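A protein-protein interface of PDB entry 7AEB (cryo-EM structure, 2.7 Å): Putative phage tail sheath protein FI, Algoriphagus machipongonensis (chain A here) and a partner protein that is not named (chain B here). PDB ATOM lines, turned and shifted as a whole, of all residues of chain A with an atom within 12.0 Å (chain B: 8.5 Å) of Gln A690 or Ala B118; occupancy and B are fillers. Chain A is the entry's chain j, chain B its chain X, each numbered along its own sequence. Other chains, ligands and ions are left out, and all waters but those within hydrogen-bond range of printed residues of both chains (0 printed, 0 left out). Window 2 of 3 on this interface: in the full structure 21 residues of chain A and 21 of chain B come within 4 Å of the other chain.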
ATOM      1  N   SER A 686      25.736  25.367  31.803  1.00  0.00           N
ATOM      2  CA  SER A 686      25.360  24.337  30.849  1.00  0.00           C
ATOM      3  C   SER A 686      25.150  25.016  29.499  1.00  0.00           C
ATOM      4  O   SER A 686      24.844  26.207  29.430  1.00  0.00           O
ATOM      5  CB  SER A 686      24.077  23.633  31.245  1.00  0.00           C
ATOM      6  OG  SER A 686      23.000  24.518  31.301  1.00  0.00           O
ATOM      7  N   HIS A 687      25.252  24.242  28.433  1.00  0.00           N
ATOM      8  CA  HIS A 687      25.177  24.778  27.093  1.00  0.00           C
ATOM      9  C   HIS A 687      24.331  23.967  26.130  1.00  0.00           C
ATOM     10  O   HIS A 687      24.032  22.811  26.358  1.00  0.00           O
ATOM     11  CB  HIS A 687      26.571  24.807  26.521  1.00  0.00           C
ATOM     12  CG  HIS A 687      26.956  23.532  25.849  1.00  0.00           C
ATOM     13  ND1 HIS A 687      27.456  22.450  26.540  1.00  0.00           N
ATOM     14  CD2 HIS A 687      26.917  23.162  24.548  1.00  0.00           C
ATOM     15  CE1 HIS A 687      27.687  21.465  25.697  1.00  0.00           C
ATOM     16  NE2 HIS A 687      27.371  21.872  24.482  1.00  0.00           N
ATOM     17  N   LYS A 688      23.952  24.625  25.039  1.00  0.00           N
ATOM     18  CA  LYS A 688      23.311  24.009  23.886  1.00  0.00           C
ATOM     19  C   LYS A 688      23.950  24.557  22.623  1.00  0.00           C
ATOM     20  O   LYS A 688      24.494  25.658  22.630  1.00  0.00           O
ATOM     21  CB  LYS A 688      21.822  24.300  23.859  1.00  0.00           C
ATOM     22  CG  LYS A 688      21.069  23.722  25.009  1.00  0.00           C
ATOM     23  CD  LYS A 688      19.590  24.004  24.887  1.00  0.00           C
ATOM     24  CE  LYS A 688      18.823  23.427  26.068  1.00  0.00           C
ATOM     25  NZ  LYS A 688      17.361  23.709  25.971  1.00  0.00           N
ATOM     26  N   MET A 689      23.881  23.795  21.538  1.00  0.00           N
ATOM     27  CA  MET A 689      24.383  24.265  20.252  1.00  0.00           C
ATOM     28  C   MET A 689      23.301  25.039  19.534  1.00  0.00           C
ATOM     29  O   MET A 689      22.127  24.680  19.606  1.00  0.00           O
ATOM     30  CB  MET A 689      24.836  23.096  19.382  1.00  0.00           C
ATOM     31  CG  MET A 689      25.961  22.268  19.971  1.00  0.00           C
ATOM     32  SD  MET A 689      27.476  23.200  20.271  1.00  0.00           S
ATOM     33  CE  MET A 689      28.067  23.564  18.626  1.00  0.00           C
ATOM     34  N   GLN A 690      23.689  26.076  18.822  1.00  0.00           N
ATOM     35  CA  GLN A 690      22.712  26.847  18.076  1.00  0.00           C
ATOM     36  C   GLN A 690      21.973  25.969  17.076  1.00  0.00           C
ATOM     37  O   GLN A 690      22.405  25.806  15.944  1.00  0.00           O
ATOM     38  CB  GLN A 690      23.387  28.018  17.369  1.00  0.00           C
ATOM     39  CG  GLN A 690      22.441  28.956  16.666  1.00  0.00           C
ATOM     40  CD  GLN A 690      23.147  30.158  16.099  1.00  0.00           C
ATOM     41  OE1 GLN A 690      24.359  30.309  16.246  1.00  0.00           O
ATOM     42  NE2 GLN A 690      22.393  31.029  15.451  1.00  0.00           N
ATOM     43  N   SER B   5      35.497  22.268  10.381  1.00  0.00           N
ATOM     44  CA  SER B   5      34.631  23.424  10.146  1.00  0.00           C
ATOM     45  C   SER B   5      34.652  24.431  11.314  1.00  0.00           C
ATOM     46  O   SER B   5      34.698  25.645  11.108  1.00  0.00           O
ATOM     47  CB  SER B   5      33.196  22.968   9.873  1.00  0.00           C
ATOM     48  OG  SER B   5      32.677  22.229  10.965  1.00  0.00           O
ATOM     49  N   LYS B   6      34.619  23.892  12.536  1.00  0.00           N
ATOM     50  CA  LYS B   6      34.606  24.655  13.782  1.00  0.00           C
ATOM     51  C   LYS B   6      36.035  24.905  14.265  1.00  0.00           C
ATOM     52  O   LYS B   6      36.440  24.427  15.315  1.00  0.00           O
ATOM     53  CB  LYS B   6      33.798  23.918  14.844  1.00  0.00           C
ATOM     54  CG  LYS B   6      32.372  23.603  14.451  1.00  0.00           C
ATOM     55  CD  LYS B   6      31.646  22.840  15.549  1.00  0.00           C
ATOM     56  CE  LYS B   6      30.226  22.496  15.135  1.00  0.00           C
ATOM     57  NZ  LYS B   6      29.502  21.743  16.195  1.00  0.00           N
ATOM     58  N   PHE B   8      37.236  28.215  14.336  1.00  0.00           N
ATOM     59  CA  PHE B   8      37.328  29.570  14.879  1.00  0.00           C
ATOM     60  C   PHE B   8      36.990  29.641  16.353  1.00  0.00           C
ATOM     61  O   PHE B   8      36.979  30.734  16.924  1.00  0.00           O
ATOM     62  CB  PHE B   8      36.489  30.610  14.085  1.00  0.00           C
ATOM     63  CG  PHE B   8      35.008  30.374  14.019  1.00  0.00           C
ATOM     64  CD1 PHE B   8      34.161  30.729  15.060  1.00  0.00           C
ATOM     65  CD2 PHE B   8      34.454  29.909  12.853  1.00  0.00           C
ATOM     66  CE1 PHE B   8      32.817  30.550  14.954  1.00  0.00           C
ATOM     67  CE2 PHE B   8      33.105  29.740  12.746  1.00  0.00           C
ATOM     68  CZ  PHE B   8      32.290  30.058  13.798  1.00  0.00           C
ATOM     69  N   LEU B   9      36.703  28.520  16.979  1.00  0.00           N
ATOM     70  CA  LEU B   9      36.541  28.545  18.413  1.00  0.00           C
ATOM     71  C   LEU B   9      37.908  28.415  19.047  1.00  0.00           C
ATOM     72  O   LEU B   9      38.144  28.923  20.148  1.00  0.00           O
ATOM     73  CB  LEU B   9      35.580  27.434  18.860  1.00  0.00           C
ATOM     74  CG  LEU B   9      34.147  27.449  18.291  1.00  0.00           C
ATOM     75  CD1 LEU B   9      33.374  26.258  18.819  1.00  0.00           C
ATOM     76  CD2 LEU B   9      33.420  28.749  18.627  1.00  0.00           C
ATOM     77  N   PRO B  89      33.409  36.435  23.832  1.00  0.00           N
ATOM     78  CA  PRO B  89      32.803  36.653  22.494  1.00  0.00           C
ATOM     79  C   PRO B  89      32.134  35.461  21.834  1.00  0.00           C
ATOM     80  O   PRO B  89      31.436  35.637  20.827  1.00  0.00           O
ATOM     81  CB  PRO B  89      34.025  37.054  21.656  1.00  0.00           C
ATOM     82  CG  PRO B  89      35.023  37.527  22.630  1.00  0.00           C
ATOM     83  CD  PRO B  89      34.844  36.711  23.832  1.00  0.00           C
ATOM     84  N   ARG B  90      32.390  34.254  22.297  1.00  0.00           N
ATOM     85  CA  ARG B  90      31.871  33.087  21.612  1.00  0.00           C
ATOM     86  C   ARG B  90      30.465  32.666  22.037  1.00  0.00           C
ATOM     87  O   ARG B  90      29.922  31.745  21.422  1.00  0.00           O
ATOM     88  CB  ARG B  90      32.862  31.929  21.778  1.00  0.00           C
ATOM     89  CG  ARG B  90      34.204  32.206  21.057  1.00  0.00           C
ATOM     90  CD  ARG B  90      35.305  31.204  21.357  1.00  0.00           C
ATOM     91  NE  ARG B  90      35.710  31.266  22.758  1.00  0.00           N
ATOM     92  CZ  ARG B  90      36.652  30.523  23.345  1.00  0.00           C
ATOM     93  NH1 ARG B  90      37.361  29.625  22.682  1.00  0.00           N
ATOM     94  NH2 ARG B  90      36.880  30.683  24.634  1.00  0.00           N
ATOM     95  N   ILE B  91      29.840  33.268  23.066  1.00  0.00           N
ATOM     96  CA  ILE B  91      28.521  32.788  23.490  1.00  0.00           C
ATOM     97  C   ILE B  91      27.471  33.882  23.648  1.00  0.00           C
ATOM     98  O   ILE B  91      27.773  35.058  23.844  1.00  0.00           O
ATOM     99  CB  ILE B  91      28.565  32.002  24.818  1.00  0.00           C
ATOM    100  CG1 ILE B  91      28.942  32.919  25.986  1.00  0.00           C
ATOM    101  CG2 ILE B  91      29.504  30.834  24.701  1.00  0.00           C
ATOM    102  CD1 ILE B  91      28.752  32.314  27.352  1.00  0.00           C
ATOM    103  N   ASP B  92      26.210  33.435  23.642  1.00  0.00           N
ATOM    104  CA  ASP B  92      25.010  34.221  23.959  1.00  0.00           C
ATOM    105  C   ASP B  92      24.279  33.594  25.139  1.00  0.00           C
ATOM    106  O   ASP B  92      23.823  32.446  25.027  1.00  0.00           O
ATOM    107  CB  ASP B  92      24.045  34.276  22.775  1.00  0.00           C
ATOM    108  CG  ASP B  92      24.465  35.212  21.677  1.00  0.00           C
ATOM    109  OD1 ASP B  92      24.610  36.412  21.916  1.00  0.00           O
ATOM    110  OD2 ASP B  92      24.655  34.738  20.550  1.00  0.00           O
ATOM    111  N   TYR B 114      23.459  28.792  28.401  1.00  0.00           N
ATOM    112  CA  TYR B 114      23.918  29.597  27.271  1.00  0.00           C
ATOM    113  C   TYR B 114      23.991  28.796  25.972  1.00  0.00           C
ATOM    114  O   TYR B 114      24.029  27.565  25.967  1.00  0.00           O
ATOM    115  CB  TYR B 114      25.287  30.221  27.559  1.00  0.00           C
ATOM    116  CG  TYR B 114      26.393  29.216  27.714  1.00  0.00           C
ATOM    117  CD1 TYR B 114      27.178  28.851  26.638  1.00  0.00           C
ATOM    118  CD2 TYR B 114      26.664  28.645  28.944  1.00  0.00           C
ATOM    119  CE1 TYR B 114      28.162  27.941  26.767  1.00  0.00           C
ATOM    120  CE2 TYR B 114      27.664  27.725  29.082  1.00  0.00           C
ATOM    121  CZ  TYR B 114      28.414  27.381  27.988  1.00  0.00           C
ATOM    122  OH  TYR B 114      29.425  26.464  28.095  1.00  0.00           O
ATOM    123  N   ILE B 115      24.112  29.543  24.870  1.00  0.00           N
ATOM    124  CA  ILE B 115      24.171  29.021  23.505  1.00  0.00           C
ATOM    125  C   ILE B 115      25.494  29.400  22.824  1.00  0.00           C
ATOM    126  O   ILE B 115      25.901  30.565  22.838  1.00  0.00           O
ATOM    127  CB  ILE B 115      22.971  29.542  22.695  1.00  0.00           C
ATOM    128  CG1 ILE B 115      21.685  29.020  23.340  1.00  0.00           C
ATOM    129  CG2 ILE B 115      23.076  29.144  21.228  1.00  0.00           C
ATOM    130  CD1 ILE B 115      20.426  29.674  22.872  1.00  0.00           C
ATOM    131  N   VAL B 116      26.142  28.420  22.197  1.00  0.00           N
ATOM    132  CA  VAL B 116      27.394  28.656  21.479  1.00  0.00           C
ATOM    133  C   VAL B 116      27.107  29.187  20.073  1.00  0.00           C
ATOM    134  O   VAL B 116      26.294  28.620  19.342  1.00  0.00           O
ATOM    135  CB  VAL B 116      28.226  27.363  21.450  1.00  0.00           C
ATOM    136  CG1 VAL B 116      29.477  27.534  20.625  1.00  0.00           C
ATOM    137  CG2 VAL B 116      28.590  26.971  22.871  1.00  0.00           C
ATOM    138  N   ARG B 117      27.777  30.280  19.694  1.00  0.00           N
ATOM    139  CA  ARG B 117      27.563  30.951  18.407  1.00  0.00           C
ATOM    140  C   ARG B 117      28.076  30.168  17.191  1.00  0.00           C
ATOM    141  O   ARG B 117      29.197  29.657  17.180  1.00  0.00           O
ATOM    142  CB  ARG B 117      28.247  32.314  18.432  1.00  0.00           C
ATOM    143  CG  ARG B 117      27.545  33.311  19.308  1.00  0.00           C
ATOM    144  CD  ARG B 117      28.299  34.588  19.431  1.00  0.00           C
ATOM    145  NE  ARG B 117      27.471  35.574  20.101  1.00  0.00           N
ATOM    146  CZ  ARG B 117      27.888  36.728  20.614  1.00  0.00           C
ATOM    147  NH1 ARG B 117      29.159  37.092  20.582  1.00  0.00           N
ATOM    148  NH2 ARG B 117      27.002  37.531  21.170  1.00  0.00           N
ATOM    149  N   ALA B 118      27.269  30.151  16.123  1.00  0.00           N
ATOM    150  CA  ALA B 118      27.615  29.490  14.865  1.00  0.00           C
ATOM    151  C   ALA B 118      28.396  30.370  13.891  1.00  0.00           C
ATOM    152  O   ALA B 118      28.799  29.887  12.830  1.00  0.00           O
ATOM    153  CB  ALA B 118      26.348  29.018  14.159  1.00  0.00           C
ATOM    154  N   THR B 119      28.532  31.660  14.170  1.00  0.00           N
ATOM    155  CA  THR B 119      29.215  32.629  13.315  1.00  0.00           C
ATOM    156  C   THR B 119      30.313  33.293  14.135  1.00  0.00           C
ATOM    157  O   THR B 119      30.182  33.364  15.339  1.00  0.00           O
ATOM    158  CB  THR B 119      28.210  33.680  12.804  1.00  0.00           C
ATOM    159  OG1 THR B 119      27.164  33.033  12.083  1.00  0.00           O
ATOM    160  CG2 THR B 119      28.837  34.706  11.897  1.00  0.00           C
ATOM    161  N   ASN B 120      31.384  33.788  13.507  1.00  0.00           N
ATOM    162  CA  ASN B 120      32.539  34.307  14.223  1.00  0.00           C
ATOM    163  C   ASN B 120      32.430  35.787  14.597  1.00  0.00           C
ATOM    164  O   ASN B 120      32.258  36.651  13.730  1.00  0.00           O
ATOM    165  CB  ASN B 120      33.799  34.075  13.419  1.00  0.00           C
ATOM    166  CG  ASN B 120      34.969  34.325  14.241  1.00  0.00           C
ATOM    167  OD1 ASN B 120      34.913  34.133  15.452  1.00  0.00           O
ATOM    168  ND2 ASN B 120      36.024  34.798  13.643  1.00  0.00           N
ATOM    169  N   SER B 121      32.569  36.061  15.894  1.00  0.00           N
ATOM    170  CA  SER B 121      32.526  37.401  16.469  1.00  0.00           C
ATOM    171  C   SER B 121      33.748  38.246  16.129  1.00  0.00           C
ATOM    172  O   SER B 121      34.868  37.750  16.037  1.00  0.00           O
ATOM    173  CB  SER B 121      32.448  37.316  17.985  1.00  0.00           C
ATOM    174  OG  SER B 121      32.620  38.604  18.524  1.00  0.00           O
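The backbone carbonyl oxygen of Ser A686 lies close to the backbone NH of Tyr B114 (3.1 Å). The backbone NH (N) of Val B116 is in hydrogen-bond range of the backbone carbonyl oxygen (O) of Lys A688, 3.2 Å away. The backbone NH (N) of Ala B118 is in hydrogen-bond range of the side-chain amide oxygen (OE1) of Gln A690 (2.9 Å). The backbone NH (N) of Lys A688 lies within hydrogen-bond range of the backbone carbonyl oxygen (O) of Tyr B114, at 3.1 Å.
NH2 of Arg B117 is in salt-bridge range of OD1 of Asp B92, at 2.7 Å. The backbone carbonyl oxygen (O) of Arg B90 is in hydrogen-bond range of the backbone NH (N) of Arg B117 (3.1 Å). The backbone carbonyl oxygen (O) of Pro B89 lies within hydrogen-bond range of the guanidinium group (NH1) of Arg B117, at 2.7 Å. The backbone carbonyl oxygen (O) of Asp B92 lies within hydrogen-bond range of the backbone NH (N) of Ile B115 (2.9 Å).
Tyr B114 touches His A687. Lys A688 touches Ile B115 (O to CA, 3.5 Å). CE of Met A689 touches NZ of Lys B6, 3.4 Å away. CG2 of Ile B115 touches CA of Gln A690, 3.9 Å away. Gln A690 touches Val B116. Gln A690 touches Arg B117 (OE1 to C, 3.8 Å).
Printed residues of chain B within 4 Å of Ser A686: Tyr B114. Printed residues of chain B within 4 Å of His A687: Tyr B114 (3.2 Å). Printed residues of chain B within 4 Å of Lys A688: Tyr B114, Ile B115 and Val B116. Gln A690 touches just these residues of chain B: Ile B115 (3.9 Å), Val B116 (3.6 Å), Arg B117 (3.8 Å) and Ala B118 (2.9 Å). Of the printed residues of chain A, Lys B6 touches Met A689 (3.4 Å). Phe B8 touches none of the printed residues of chain A. Of chain A, only Lys A688 and Gln A690 come within 4 Å of Ile B115. Of chain A, only Lys A688 and Gln A690 come within 4 Å of Val B116. Of the printed residues of chain A, Arg B117 touches Gln A690. No residue of chain A comes within 4 Å of Thr B119. The nearest residue of chain A that does not touch Ala B118 is Met A689 (7.0 Å).
Printed residues of chain B that touch a printed residue of chain A: Lys B6, Tyr B114, Ile B115, Val B116, Arg B117 and Ala B118. Along chain B the printed residues that touch a printed residue of chain A span positions 6 to 118. Of the 5 printed residues of chain A, 5 touch a printed residue of chain B. Hydrophobic or aromatic side chains of chain A that line the printed part of chain B: His A687 and Met A689. Among the printed residues, no Asp or Glu carboxylate lies within 4 Å of a Lys or Arg side-chain nitrogen of the other chain.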
